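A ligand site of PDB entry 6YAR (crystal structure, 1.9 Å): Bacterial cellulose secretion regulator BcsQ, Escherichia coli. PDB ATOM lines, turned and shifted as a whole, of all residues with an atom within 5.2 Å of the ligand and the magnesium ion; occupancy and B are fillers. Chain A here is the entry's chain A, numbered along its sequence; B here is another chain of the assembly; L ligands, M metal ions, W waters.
The side-chain carboxylate (OD2) of Asp 124 sits close to the side-chain hydroxyl (OG1) of Thr 16 (2.5 Å). OD1 of Asn 152 of chain B sits at hydrogen-bond distance from NE of Arg 156 of chain B (2.8 Å). NH1 of Arg 156 of chain B is in salt-bridge range of OD1 of Asp 41, at 3.2 Å. OD1 of Asp 150 of chain B sits at hydrogen-bond distance from N of Asn 152 of chain B, at 3.1 Å. OD1 of Asn 152 of chain B sits close to NH1 of Arg 10 of chain B, at 3.3 Å. The side-chain amide nitrogen (ND2) of Asn 171 sits at hydrogen-bond distance from the backbone carbonyl oxygen (O) of Val 13 (2.8 Å). OD2 of Asp 150 of chain B is in salt-bridge range of NH2 of Arg 10 of chain B (2.7 Å). N of Asn 172 sits at hydrogen-bond distance from O of Ile 199 (2.9 Å).
Water W2 bridges O7 of the ligand and ND2 of Asn 152 of chain B. Water W7 lies within hydrogen-bond range of the side-chain carboxylate of Asp 124 (2.6 Å) and the side-chain sulfur of Cys 39 (3.4 Å). Water W4 lies within hydrogen-bond range of the side-chain carboxylate of Asp 41 (2.6 Å) and the side-chain sulfur of Cys 39 (3.7 Å). Water W6 bridges O1 of the ligand (2.7 Å) and N of Gly 11 of chain B (2.8 Å). Water W5 lies within hydrogen-bond range of an oxygen (O4) of the ligand (2.7 Å), the side-chain hydroxyl of Thr 15 (2.9 Å) and the backbone carbonyl oxygen of Arg 10 of chain A (3.0 Å). Water W1 lies within hydrogen-bond range of N of Ala 151 of chain B (2.8 Å), O of Ala 206 (2.9 Å) and O12 of the ligand (3.0 Å).
CA of Gly 11 of chain A touches O1 of the ligand (3.4 Å). Leu 43 touches the ligand (CD1 to O2, 3.7 Å). Asn 172 touches the ligand. CA of Arg 201 touches N4 of the ligand, at 3.5 Å. CA of Ala 206 touches O13 of the ligand, at 3.4 Å. CD of Arg 10 of chain B touches O2 of the ligand, at 3.8 Å. Asp 150 of chain B touches the ligand (CB to O12, 3.2 Å). Hydrophobic or aromatic side chains that line the ligand: Val 13, Leu 43, Met 205 and Ala 206. 20 residues have an atom within 4 Å of the ligand: Gly 11 of chain A, Gly 12, Val 13, Gly 14, Thr 15, Thr 16, Thr 17, Leu 43, Asn 171, Asn 172, His 200, Arg 201, Asp 202, Met 205, Ala 206, Arg 10 of chain B, Asp 150 of chain B, Ala 151 of chain B, Asn 152 of chain B and Arg 156 of chain B.
N of Thr 16 sits at hydrogen-bond distance from O8 of the ligand (3.3 Å). The backbone NH (N) of Thr 17 is in hydrogen-bond range of an oxygen (O8) of the ligand (2.7 Å). O8 of the ligand lies within hydrogen-bond range of OG1 of Thr 17, at 2.6 Å. The guanidinium group of Arg 156 of chain B lies within salt-bridge range of an oxygen (O2) of the ligand, 2.6 Å away. An oxygen (O13) of the ligand sits at hydrogen-bond distance from the backbone carbonyl oxygen of Met 205 (2.7 Å). An oxygen (O12) of the ligand sits at hydrogen-bond distance from the backbone NH (N) of Asn 152 of chain B. ND2 of Asn 152 of chain B is in hydrogen-bond range of O2 of the ligand (2.8 Å). An oxygen (O1) of the ligand lies within hydrogen-bond range of the backbone NH (N) of Gly 12, 2.8 Å away. A nitrogen (N2) of the ligand sits at hydrogen-bond distance from the side-chain amide nitrogen (ND2) of Asn 171 (2.9 Å). N of Gly 14 sits at hydrogen-bond distance from O4 of the ligand (3.0 Å). N4 of the ligand sits at hydrogen-bond distance from N of Asp 202, 3.0 Å away. The backbone NH of Val 13 lies within hydrogen-bond range of an oxygen (O4) of the ligand (3.0 Å). A nitrogen (N3) of the ligand sits at hydrogen-bond distance from the backbone carbonyl oxygen (O) of His 200 (3.1 Å). An oxygen (O4) of the ligand is in hydrogen-bond range of the backbone NH (N) of Thr 15 (3.1 Å). An oxygen (O12) of the ligand is in hydrogen-bond range of the backbone NH (N) of Ala 151 of chain B (3.5 Å).
Within 4 Å of the magnesium ion: Thr 16. The nearest printed residue that does not touch the magnesium ion is Asp 124 (4.1 Å).
The magnesium ion is bound by water W8 (2.0 Å), an oxygen (O3) of the ligand (2.1 Å), water W2 (2.1 Å), the side-chain hydroxyl of Thr 16 (2.1 Å), an oxygen (O5) of the ligand (2.2 Å) and water W7 (2.3 Å).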
ATOM      1  N   ARG A  10      27.987  17.262 -26.361  1.00  0.00           N
ATOM      2  CA  ARG A  10      27.688  16.485 -25.167  1.00  0.00           C
ATOM      3  C   ARG A  10      27.271  17.461 -24.081  1.00  0.00           C
ATOM      4  O   ARG A  10      27.254  18.679 -24.282  1.00  0.00           O
ATOM      5  CB  ARG A  10      28.870  15.616 -24.749  1.00  0.00           C
ATOM      6  CG  ARG A  10      30.141  16.344 -24.481  1.00  0.00           C
ATOM      7  CD  ARG A  10      30.952  15.716 -23.322  1.00  0.00           C
ATOM      8  NE  ARG A  10      31.792  16.762 -22.752  1.00  0.00           N
ATOM      9  CZ  ARG A  10      33.076  16.948 -23.040  1.00  0.00           C
ATOM     10  NH1 ARG A  10      33.723  16.103 -23.841  1.00  0.00           N
ATOM     11  NH2 ARG A  10      33.725  17.983 -22.497  1.00  0.00           N
ATOM     12  N   GLY A  11      26.880  16.915 -22.929  1.00  0.00           N
ATOM     13  CA  GLY A  11      26.499  17.752 -21.819  1.00  0.00           C
ATOM     14  C   GLY A  11      27.672  18.538 -21.260  1.00  0.00           C
ATOM     15  O   GLY A  11      28.833  18.142 -21.381  1.00  0.00           O
ATOM     16  N   GLY A  12      27.352  19.690 -20.683  1.00  0.00           N
ATOM     17  CA  GLY A  12      28.335  20.473 -19.940  1.00  0.00           C
ATOM     18  C   GLY A  12      29.309  21.295 -20.769  1.00  0.00           C
ATOM     19  O   GLY A  12      30.220  21.891 -20.188  1.00  0.00           O
ATOM     20  N   VAL A  13      29.157  21.362 -22.093  1.00  0.00           N
ATOM     21  CA  VAL A  13      30.128  22.106 -22.895  1.00  0.00           C
ATOM     22  C   VAL A  13      29.932  23.613 -22.888  1.00  0.00           C
ATOM     23  O   VAL A  13      30.830  24.326 -23.364  1.00  0.00           O
ATOM     24  CB  VAL A  13      30.159  21.603 -24.342  1.00  0.00           C
ATOM     25  CG1 VAL A  13      30.708  20.148 -24.375  1.00  0.00           C
ATOM     26  CG2 VAL A  13      28.754  21.685 -24.976  1.00  0.00           C
ATOM     27  N   GLY A  14      28.827  24.121 -22.349  1.00  0.00           N
ATOM     28  CA  GLY A  14      28.651  25.578 -22.233  1.00  0.00           C
ATOM     29  C   GLY A  14      27.494  26.153 -23.045  1.00  0.00           C
ATOM     30  O   GLY A  14      27.390  27.376 -23.209  1.00  0.00           O
ATOM     31  N   THR A  15      26.608  25.276 -23.529  1.00  0.00           N
ATOM     32  CA  THR A  15      25.547  25.672 -24.457  1.00  0.00           C
ATOM     33  C   THR A  15      24.630  26.718 -23.845  1.00  0.00           C
ATOM     34  O   THR A  15      24.305  27.730 -24.477  1.00  0.00           O
ATOM     35  CB  THR A  15      24.736  24.427 -24.866  1.00  0.00           C
ATOM     36  OG1 THR A  15      25.629  23.430 -25.375  1.00  0.00           O
ATOM     37  CG2 THR A  15      23.735  24.784 -25.943  1.00  0.00           C
ATOM     38  N   THR A  16      24.191  26.506 -22.598  1.00  0.00           N
ATOM     39  CA  THR A  16      23.226  27.421 -22.004  1.00  0.00           C
ATOM     40  C   THR A  16      23.844  28.794 -21.726  1.00  0.00           C
ATOM     41  O   THR A  16      23.232  29.836 -22.005  1.00  0.00           O
ATOM     42  CB  THR A  16      22.653  26.817 -20.731  1.00  0.00           C
ATOM     43  OG1 THR A  16      21.889  25.655 -21.054  1.00  0.00           O
ATOM     44  CG2 THR A  16      21.769  27.818 -20.010  1.00  0.00           C
ATOM     45  N   THR A  17      25.074  28.809 -21.193  1.00  0.00           N
ATOM     46  CA  THR A  17      25.746  30.083 -20.947  1.00  0.00           C
ATOM     47  C   THR A  17      25.979  30.831 -22.255  1.00  0.00           C
ATOM     48  O   THR A  17      25.800  32.060 -22.321  1.00  0.00           O
ATOM     49  CB  THR A  17      27.073  29.855 -20.223  1.00  0.00           C
ATOM     50  OG1 THR A  17      26.854  29.012 -19.089  1.00  0.00           O
ATOM     51  CG2 THR A  17      27.640  31.194 -19.737  1.00  0.00           C
ATOM     52  N   ILE A  18      26.379  30.113 -23.299  1.00  0.00           N
ATOM     53  CA  ILE A  18      26.572  30.748 -24.603  1.00  0.00           C
ATOM     54  C   ILE A  18      25.251  31.260 -25.173  1.00  0.00           C
ATOM     55  O   ILE A  18      25.209  32.341 -25.783  1.00  0.00           O
ATOM     56  CB  ILE A  18      27.270  29.768 -25.560  1.00  0.00           C
ATOM     57  CG1 ILE A  18      28.701  29.499 -25.094  1.00  0.00           C
ATOM     58  CG2 ILE A  18      27.195  30.270 -27.030  1.00  0.00           C
ATOM     59  CD1 ILE A  18      29.367  28.355 -25.829  1.00  0.00           C
ATOM     60  N   CYS A  39      15.445  22.722 -22.817  1.00  0.00           N
ATOM     61  CA  CYS A  39      16.026  21.700 -21.946  1.00  0.00           C
ATOM     62  C   CYS A  39      15.153  21.499 -20.723  1.00  0.00           C
ATOM     63  O   CYS A  39      14.787  22.478 -20.046  1.00  0.00           O
ATOM     64  CB  CYS A  39      17.433  22.102 -21.508  1.00  0.00           C
ATOM     65  SG  CYS A  39      18.566  22.317 -22.892  1.00  0.00           S
ATOM     66  N   ASP A  41      16.042  20.477 -17.908  1.00  0.00           N
ATOM     67  CA  ASP A  41      16.782  21.025 -16.765  1.00  0.00           C
ATOM     68  C   ASP A  41      16.298  22.416 -16.372  1.00  0.00           C
ATOM     69  O   ASP A  41      16.394  22.803 -15.198  1.00  0.00           O
ATOM     70  CB  ASP A  41      18.281  21.127 -17.080  1.00  0.00           C
ATOM     71  CG  ASP A  41      18.810  19.925 -17.843  1.00  0.00           C
ATOM     72  OD1 ASP A  41      18.850  18.815 -17.275  1.00  0.00           O
ATOM     73  OD2 ASP A  41      19.202  20.131 -19.012  1.00  0.00           O
ATOM     74  N   LEU A  43      17.457  25.424 -16.936  1.00  0.00           N
ATOM     75  CA  LEU A  43      18.549  26.202 -16.351  1.00  0.00           C
ATOM     76  C   LEU A  43      18.720  27.583 -16.978  1.00  0.00           C
ATOM     77  O   LEU A  43      19.243  28.490 -16.305  1.00  0.00           O
ATOM     78  CB  LEU A  43      19.868  25.427 -16.485  1.00  0.00           C
ATOM     79  CG  LEU A  43      19.868  24.062 -15.770  1.00  0.00           C
ATOM     80  CD1 LEU A  43      21.073  23.171 -16.185  1.00  0.00           C
ATOM     81  CD2 LEU A  43      19.856  24.291 -14.277  1.00  0.00           C
ATOM     82  N   ASP A 124      17.920  27.026 -26.790  1.00  0.00           N
ATOM     83  CA  ASP A 124      18.835  26.179 -26.039  1.00  0.00           C
ATOM     84  C   ASP A 124      18.281  24.761 -26.078  1.00  0.00           C
ATOM     85  O   ASP A 124      17.237  24.480 -25.485  1.00  0.00           O
ATOM     86  CB  ASP A 124      18.943  26.720 -24.617  1.00  0.00           C
ATOM     87  CG  ASP A 124      19.921  25.946 -23.720  1.00  0.00           C
ATOM     88  OD1 ASP A 124      20.583  24.971 -24.147  1.00  0.00           O
ATOM     89  OD2 ASP A 124      19.994  26.354 -22.546  1.00  0.00           O
ATOM     90  N   ASN A 171      34.099  26.093 -27.144  1.00  0.00           N
ATOM     91  CA  ASN A 171      34.000  26.827 -25.899  1.00  0.00           C
ATOM     92  C   ASN A 171      35.033  26.298 -24.929  1.00  0.00           C
ATOM     93  O   ASN A 171      35.547  25.173 -25.067  1.00  0.00           O
ATOM     94  CB  ASN A 171      32.590  26.710 -25.281  1.00  0.00           C
ATOM     95  CG  ASN A 171      32.445  27.539 -24.003  1.00  0.00           C
ATOM     96  OD1 ASN A 171      32.824  28.717 -23.962  1.00  0.00           O
ATOM     97  ND2 ASN A 171      31.921  26.917 -22.949  1.00  0.00           N
ATOM     98  N   ASN A 172      35.351  27.123 -23.926  1.00  0.00           N
ATOM     99  CA  ASN A 172      36.150  26.733 -22.786  1.00  0.00           C
ATOM    100  C   ASN A 172      37.598  26.455 -23.162  1.00  0.00           C
ATOM    101  O   ASN A 172      38.281  25.675 -22.506  1.00  0.00           O
ATOM    102  CB  ASN A 172      35.554  25.505 -22.075  1.00  0.00           C
ATOM    103  CG  ASN A 172      35.408  25.706 -20.578  1.00  0.00           C
ATOM    104  OD1 ASN A 172      36.234  26.358 -19.947  1.00  0.00           O
ATOM    105  ND2 ASN A 172      34.334  25.165 -20.009  1.00  0.00           N
ATOM    106  N   ILE A 199      35.309  30.637 -28.022  1.00  0.00           N
ATOM    107  CA  ILE A 199      35.136  31.235 -26.696  1.00  0.00           C
ATOM    108  C   ILE A 199      36.182  30.636 -25.759  1.00  0.00           C
ATOM    109  O   ILE A 199      36.199  29.416 -25.548  1.00  0.00           O
ATOM    110  CB  ILE A 199      33.714  31.017 -26.154  1.00  0.00           C
ATOM    111  CG1 ILE A 199      32.659  31.278 -27.228  1.00  0.00           C
ATOM    112  CG2 ILE A 199      33.476  31.881 -24.917  1.00  0.00           C
ATOM    113  CD1 ILE A 199      32.749  32.651 -27.849  1.00  0.00           C
ATOM    114  N   HIS A 200      37.049  31.473 -25.218  1.00  0.00           N
ATOM    115  CA  HIS A 200      38.055  31.003 -24.285  1.00  0.00           C
ATOM    116  C   HIS A 200      37.430  30.649 -22.931  1.00  0.00           C
ATOM    117  O   HIS A 200      36.376  31.167 -22.561  1.00  0.00           O
ATOM    118  CB  HIS A 200      39.145  32.057 -24.067  1.00  0.00           C
ATOM    119  CG  HIS A 200      40.180  32.110 -25.151  1.00  0.00           C
ATOM    120  ND1 HIS A 200      40.038  32.885 -26.280  1.00  0.00           N
ATOM    121  CD2 HIS A 200      41.367  31.482 -25.263  1.00  0.00           C
ATOM    122  CE1 HIS A 200      41.100  32.739 -27.043  1.00  0.00           C
ATOM    123  NE2 HIS A 200      41.927  31.889 -26.456  1.00  0.00           N
ATOM    124  N   ARG A 201      38.088  29.744 -22.203  1.00  0.00           N
ATOM    125  CA  ARG A 201      37.813  29.633 -20.775  1.00  0.00           C
ATOM    126  C   ARG A 201      38.007  31.000 -20.140  1.00  0.00           C
ATOM    127  O   ARG A 201      38.984  31.698 -20.423  1.00  0.00           O
ATOM    128  CB  ARG A 201      38.729  28.594 -20.114  1.00  0.00           C
ATOM    129  CG  ARG A 201      38.293  28.248 -18.683  1.00  0.00           C
ATOM    130  CD  ARG A 201      39.143  27.133 -18.078  1.00  0.00           C
ATOM    131  NE  ARG A 201      40.316  27.704 -17.420  1.00  0.00           N
ATOM    132  CZ  ARG A 201      41.247  26.990 -16.782  1.00  0.00           C
ATOM    133  NH1 ARG A 201      41.152  25.665 -16.710  1.00  0.00           N
ATOM    134  NH2 ARG A 201      42.269  27.612 -16.206  1.00  0.00           N
ATOM    135  N   ASP A 202      37.084  31.383 -19.271  1.00  0.00           N
ATOM    136  CA  ASP A 202      37.066  32.740 -18.714  1.00  0.00           C
ATOM    137  C   ASP A 202      36.243  32.700 -17.441  1.00  0.00           C
ATOM    138  O   ASP A 202      35.087  32.256 -17.461  1.00  0.00           O
ATOM    139  CB  ASP A 202      36.469  33.724 -19.737  1.00  0.00           C
ATOM    140  CG  ASP A 202      36.623  35.167 -19.320  1.00  0.00           C
ATOM    141  OD1 ASP A 202      36.497  35.453 -18.108  1.00  0.00           O
ATOM    142  OD2 ASP A 202      36.885  36.016 -20.191  1.00  0.00           O
ATOM    143  N   GLU A 203      36.813  33.163 -16.337  1.00  0.00           N
ATOM    144  CA  GLU A 203      36.071  33.131 -15.081  1.00  0.00           C
ATOM    145  C   GLU A 203      34.813  33.989 -15.131  1.00  0.00           C
ATOM    146  O   GLU A 203      33.885  33.753 -14.353  1.00  0.00           O
ATOM    147  CB  GLU A 203      36.995  33.552 -13.928  1.00  0.00           C
ATOM    148  CG  GLU A 203      38.054  32.504 -13.603  1.00  0.00           C
ATOM    149  CD  GLU A 203      37.444  31.138 -13.390  1.00  0.00           C
ATOM    150  OE1 GLU A 203      36.549  31.025 -12.524  1.00  0.00           O
ATOM    151  OE2 GLU A 203      37.842  30.180 -14.105  1.00  0.00           O
ATOM    152  N   MET A 205      32.690  33.725 -17.480  1.00  0.00           N
ATOM    153  CA  MET A 205      31.727  32.703 -17.893  1.00  0.00           C
ATOM    154  C   MET A 205      31.385  31.708 -16.781  1.00  0.00           C
ATOM    155  O   MET A 205      30.317  31.093 -16.807  1.00  0.00           O
ATOM    156  CB  MET A 205      32.239  31.911 -19.097  1.00  0.00           C
ATOM    157  CG  MET A 205      32.422  32.745 -20.352  1.00  0.00           C
ATOM    158  SD  MET A 205      30.729  33.032 -21.296  1.00  0.00           S
ATOM    159  CE  MET A 205      30.424  31.177 -21.928  1.00  0.00           C
ATOM    160  N   ALA A 206      32.299  31.521 -15.838  1.00  0.00           N
ATOM    161  CA  ALA A 206      31.975  30.712 -14.666  1.00  0.00           C
ATOM    162  C   ALA A 206      31.192  31.506 -13.642  1.00  0.00           C
ATOM    163  O   ALA A 206      30.290  30.959 -12.988  1.00  0.00           O
ATOM    164  CB  ALA A 206      33.255  30.159 -14.030  1.00  0.00           C
ATOM    165  N   GLU A 207      31.492  32.802 -13.508  1.00  0.00           N
ATOM    166  CA  GLU A 207      30.890  33.633 -12.466  1.00  0.00           C
ATOM    167  C   GLU A 207      29.522  34.166 -12.856  1.00  0.00           C
ATOM    168  O   GLU A 207      28.672  34.372 -11.973  1.00  0.00           O
ATOM    169  CB  GLU A 207      31.819  34.821 -12.166  1.00  0.00           C
ATOM    170  CG  GLU A 207      33.099  34.393 -11.432  1.00  0.00           C
ATOM    171  CD  GLU A 207      34.123  35.518 -11.323  1.00  0.00           C
ATOM    172  OE1 GLU A 207      33.789  36.689 -11.647  1.00  0.00           O
ATOM    173  OE2 GLU A 207      35.253  35.212 -10.929  1.00  0.00           O
ATOM    174  N   LEU A 209      26.854  32.989 -14.266  1.00  0.00           N
ATOM    175  CA  LEU A 209      25.723  32.174 -13.823  1.00  0.00           C
ATOM    176  C   LEU A 209      25.489  32.326 -12.320  1.00  0.00           C
ATOM    177  O   LEU A 209      24.333  32.402 -11.875  1.00  0.00           O
ATOM    178  CB  LEU A 209      25.927  30.699 -14.189  1.00  0.00           C
ATOM    179  CG  LEU A 209      24.848  29.657 -13.826  1.00  0.00           C
ATOM    180  CD1 LEU A 209      23.464  30.081 -14.292  1.00  0.00           C
ATOM    181  CD2 LEU A 209      25.180  28.291 -14.412  1.00  0.00           C
ATOM    182  N   ARG B  10      25.443  15.669 -14.664  1.00  0.00           N
ATOM    183  CA  ARG B  10      25.203  16.172 -16.010  1.00  0.00           C
ATOM    184  C   ARG B  10      26.300  15.567 -16.864  1.00  0.00           C
ATOM    185  O   ARG B  10      27.236  14.957 -16.352  1.00  0.00           O
ATOM    186  CB  ARG B  10      25.228  17.705 -16.084  1.00  0.00           C
ATOM    187  CG  ARG B  10      26.583  18.306 -15.808  1.00  0.00           C
ATOM    188  CD  ARG B  10      26.838  19.625 -16.576  1.00  0.00           C
ATOM    189  NE  ARG B  10      28.272  19.909 -16.544  1.00  0.00           N
ATOM    190  CZ  ARG B  10      28.832  20.779 -15.721  1.00  0.00           C
ATOM    191  NH1 ARG B  10      28.090  21.489 -14.880  1.00  0.00           N
ATOM    192  NH2 ARG B  10      30.152  20.954 -15.738  1.00  0.00           N
ATOM    193  N   GLY B  11      26.178  15.750 -18.181  1.00  0.00           N
ATOM    194  CA  GLY B  11      27.163  15.187 -19.078  1.00  0.00           C
ATOM    195  C   GLY B  11      28.530  15.835 -18.920  1.00  0.00           C
ATOM    196  O   GLY B  11      28.672  16.960 -18.449  1.00  0.00           O
ATOM    197  N   ASP B 150      30.892  23.728 -10.067  1.00  0.00           N
ATOM    198  CA  ASP B 150      30.517  24.893 -10.844  1.00  0.00           C
ATOM    199  C   ASP B 150      29.052  25.205 -10.537  1.00  0.00           C
ATOM    200  O   ASP B 150      28.357  24.411  -9.889  1.00  0.00           O
ATOM    201  CB  ASP B 150      30.775  24.697 -12.348  1.00  0.00           C
ATOM    202  CG  ASP B 150      30.023  23.481 -12.944  1.00  0.00           C
ATOM    203  OD1 ASP B 150      28.812  23.285 -12.664  1.00  0.00           O
ATOM    204  OD2 ASP B 150      30.648  22.732 -13.721  1.00  0.00           O
ATOM    205  N   ALA B 151      28.608  26.369 -10.996  1.00  0.00           N
ATOM    206  CA  ALA B 151      27.245  26.811 -10.679  1.00  0.00           C
ATOM    207  C   ALA B 151      26.192  25.874 -11.282  1.00  0.00           C
ATOM    208  O   ALA B 151      25.121  25.682 -10.686  1.00  0.00           O
ATOM    209  CB  ALA B 151      27.046  28.251 -11.176  1.00  0.00           C
ATOM    210  N   ASN B 152      26.479  25.292 -12.443  1.00  0.00           N
ATOM    211  CA  ASN B 152      25.543  24.348 -13.062  1.00  0.00           C
ATOM    212  C   ASN B 152      25.291  23.160 -12.137  1.00  0.00           C
ATOM    213  O   ASN B 152      24.148  22.924 -11.726  1.00  0.00           O
ATOM    214  CB  ASN B 152      26.096  23.933 -14.436  1.00  0.00           C
ATOM    215  CG  ASN B 152      25.233  22.884 -15.137  1.00  0.00           C
ATOM    216  OD1 ASN B 152      24.826  21.876 -14.550  1.00  0.00           O
ATOM    217  ND2 ASN B 152      24.994  23.098 -16.437  1.00  0.00           N
ATOM    218  N   ARG B 156      21.833  21.898 -10.101  1.00  0.00           N
ATOM    219  CA  ARG B 156      21.287  20.565 -10.315  1.00  0.00           C
ATOM    220  C   ARG B 156      21.089  19.822  -8.996  1.00  0.00           C
ATOM    221  O   ARG B 156      20.073  19.158  -8.802  1.00  0.00           O
ATOM    222  CB  ARG B 156      22.188  19.768 -11.266  1.00  0.00           C
ATOM    223  CG  ARG B 156      22.192  20.298 -12.692  1.00  0.00           C
ATOM    224  CD  ARG B 156      23.101  19.472 -13.584  1.00  0.00           C
ATOM    225  NE  ARG B 156      22.941  19.811 -14.995  1.00  0.00           N
ATOM    226  CZ  ARG B 156      22.056  19.218 -15.795  1.00  0.00           C
ATOM    227  NH1 ARG B 156      21.265  18.258 -15.308  1.00  0.00           N
ATOM    228  NH2 ARG B 156      21.944  19.592 -17.063  1.00  0.00           N
ATOM    229  N   ARG B 174      40.159  22.571  -9.994  1.00  0.00           N
ATOM    230  CA  ARG B 174      41.275  23.251 -10.634  1.00  0.00           C
ATOM    231  C   ARG B 174      41.661  24.511  -9.868  1.00  0.00           C
ATOM    232  O   ARG B 174      40.962  24.977  -8.957  1.00  0.00           O
ATOM    233  CB  ARG B 174      40.970  23.582 -12.091  1.00  0.00           C
ATOM    234  CG  ARG B 174      39.851  24.550 -12.291  1.00  0.00           C
ATOM    235  CD  ARG B 174      39.732  24.929 -13.759  1.00  0.00           C
ATOM    236  NE  ARG B 174      38.538  25.728 -14.020  1.00  0.00           N
ATOM    237  CZ  ARG B 174      38.489  27.053 -13.957  1.00  0.00           C
ATOM    238  NH1 ARG B 174      39.593  27.754 -13.635  1.00  0.00           N
ATOM    239  NH2 ARG B 174      37.350  27.683 -14.204  1.00  0.00           N
HETATM  240  P1  LIG L   1      24.091  21.220 -19.515  1.00  0.00           P
HETATM  241  O1  LIG L   1      24.605  19.918 -19.983  1.00  0.00           O
HETATM  242  O2  LIG L   1      23.701  21.268 -18.033  1.00  0.00           O
HETATM  243  O3  LIG L   1      22.928  21.710 -20.332  1.00  0.00           O
HETATM  244  P2  LIG L   1      25.731  23.211 -20.815  1.00  0.00           P
HETATM  245  O4  LIG L   1      26.354  22.544 -21.989  1.00  0.00           O
HETATM  246  O5  LIG L   1      24.504  24.008 -21.167  1.00  0.00           O
HETATM  247  O6  LIG L   1      25.282  22.272 -19.624  1.00  0.00           O
HETATM  248  P3  LIG L   1      26.550  25.474 -19.183  1.00  0.00           P
HETATM  249  O7  LIG L   1      25.489  25.240 -18.189  1.00  0.00           O
HETATM  250  O8  LIG L   1      26.434  26.674 -20.120  1.00  0.00           O
HETATM  251  O9  LIG L   1      26.747  24.190 -20.091  1.00  0.00           O
HETATM  252  O10 LIG L   1      27.986  25.537 -18.471  1.00  0.00           O
HETATM  253  C1  LIG L   1      28.399  24.531 -17.515  1.00  0.00           C
HETATM  254  C2  LIG L   1      29.323  25.193 -16.530  1.00  0.00           C
HETATM  255  O11 LIG L   1      30.522  25.641 -17.219  1.00  0.00           O
HETATM  256  C3  LIG L   1      28.736  26.436 -15.837  1.00  0.00           C
HETATM  257  O12 LIG L   1      29.071  26.482 -14.461  1.00  0.00           O
HETATM  258  C4  LIG L   1      29.378  27.591 -16.600  1.00  0.00           C
HETATM  259  O13 LIG L   1      29.479  28.757 -15.788  1.00  0.00           O
HETATM  260  C5  LIG L   1      30.743  27.010 -16.974  1.00  0.00           C
HETATM  261  N1  LIG L   1      31.302  27.583 -18.189  1.00  0.00           N
HETATM  262  C6  LIG L   1      30.729  27.548 -19.432  1.00  0.00           C
HETATM  263  N2  LIG L   1      31.454  28.083 -20.373  1.00  0.00           N
HETATM  264  C7  LIG L   1      32.591  28.527 -19.702  1.00  0.00           C
HETATM  265  C8  LIG L   1      33.745  29.198 -20.131  1.00  0.00           C
HETATM  266  N3  LIG L   1      33.979  29.537 -21.409  1.00  0.00           N
HETATM  267  N4  LIG L   1      34.681  29.518 -19.202  1.00  0.00           N
HETATM  268  C9  LIG L   1      34.461  29.162 -17.935  1.00  0.00           C
HETATM  269  N5  LIG L   1      33.411  28.504 -17.412  1.00  0.00           N
HETATM  270  C10 LIG L   1      32.506  28.226 -18.357  1.00  0.00           C
HETATM  271 MG    MG M   1      22.402  23.670 -20.633  1.00  0.00          MG
HETATM  272  O   HOH W   1      30.343  28.134 -12.344  1.00  0.00           O
HETATM  273  O   HOH W   2      23.043  24.284 -18.779  1.00  0.00           O
HETATM  274  O   HOH W   3      33.754  26.627 -15.078  1.00  0.00           O
HETATM  275  O   HOH W   4      20.888  20.242 -20.953  1.00  0.00           O
HETATM  276  O   HOH W   5      25.317  20.958 -23.885  1.00  0.00           O
HETATM  277  O   HOH W   6      24.243  17.339 -19.380  1.00  0.00           O
HETATM  278  O   HOH W   7      21.866  23.159 -22.760  1.00  0.00           O
HETATM  279  O   HOH W   8      20.461  23.200 -20.201  1.00  0.00           O
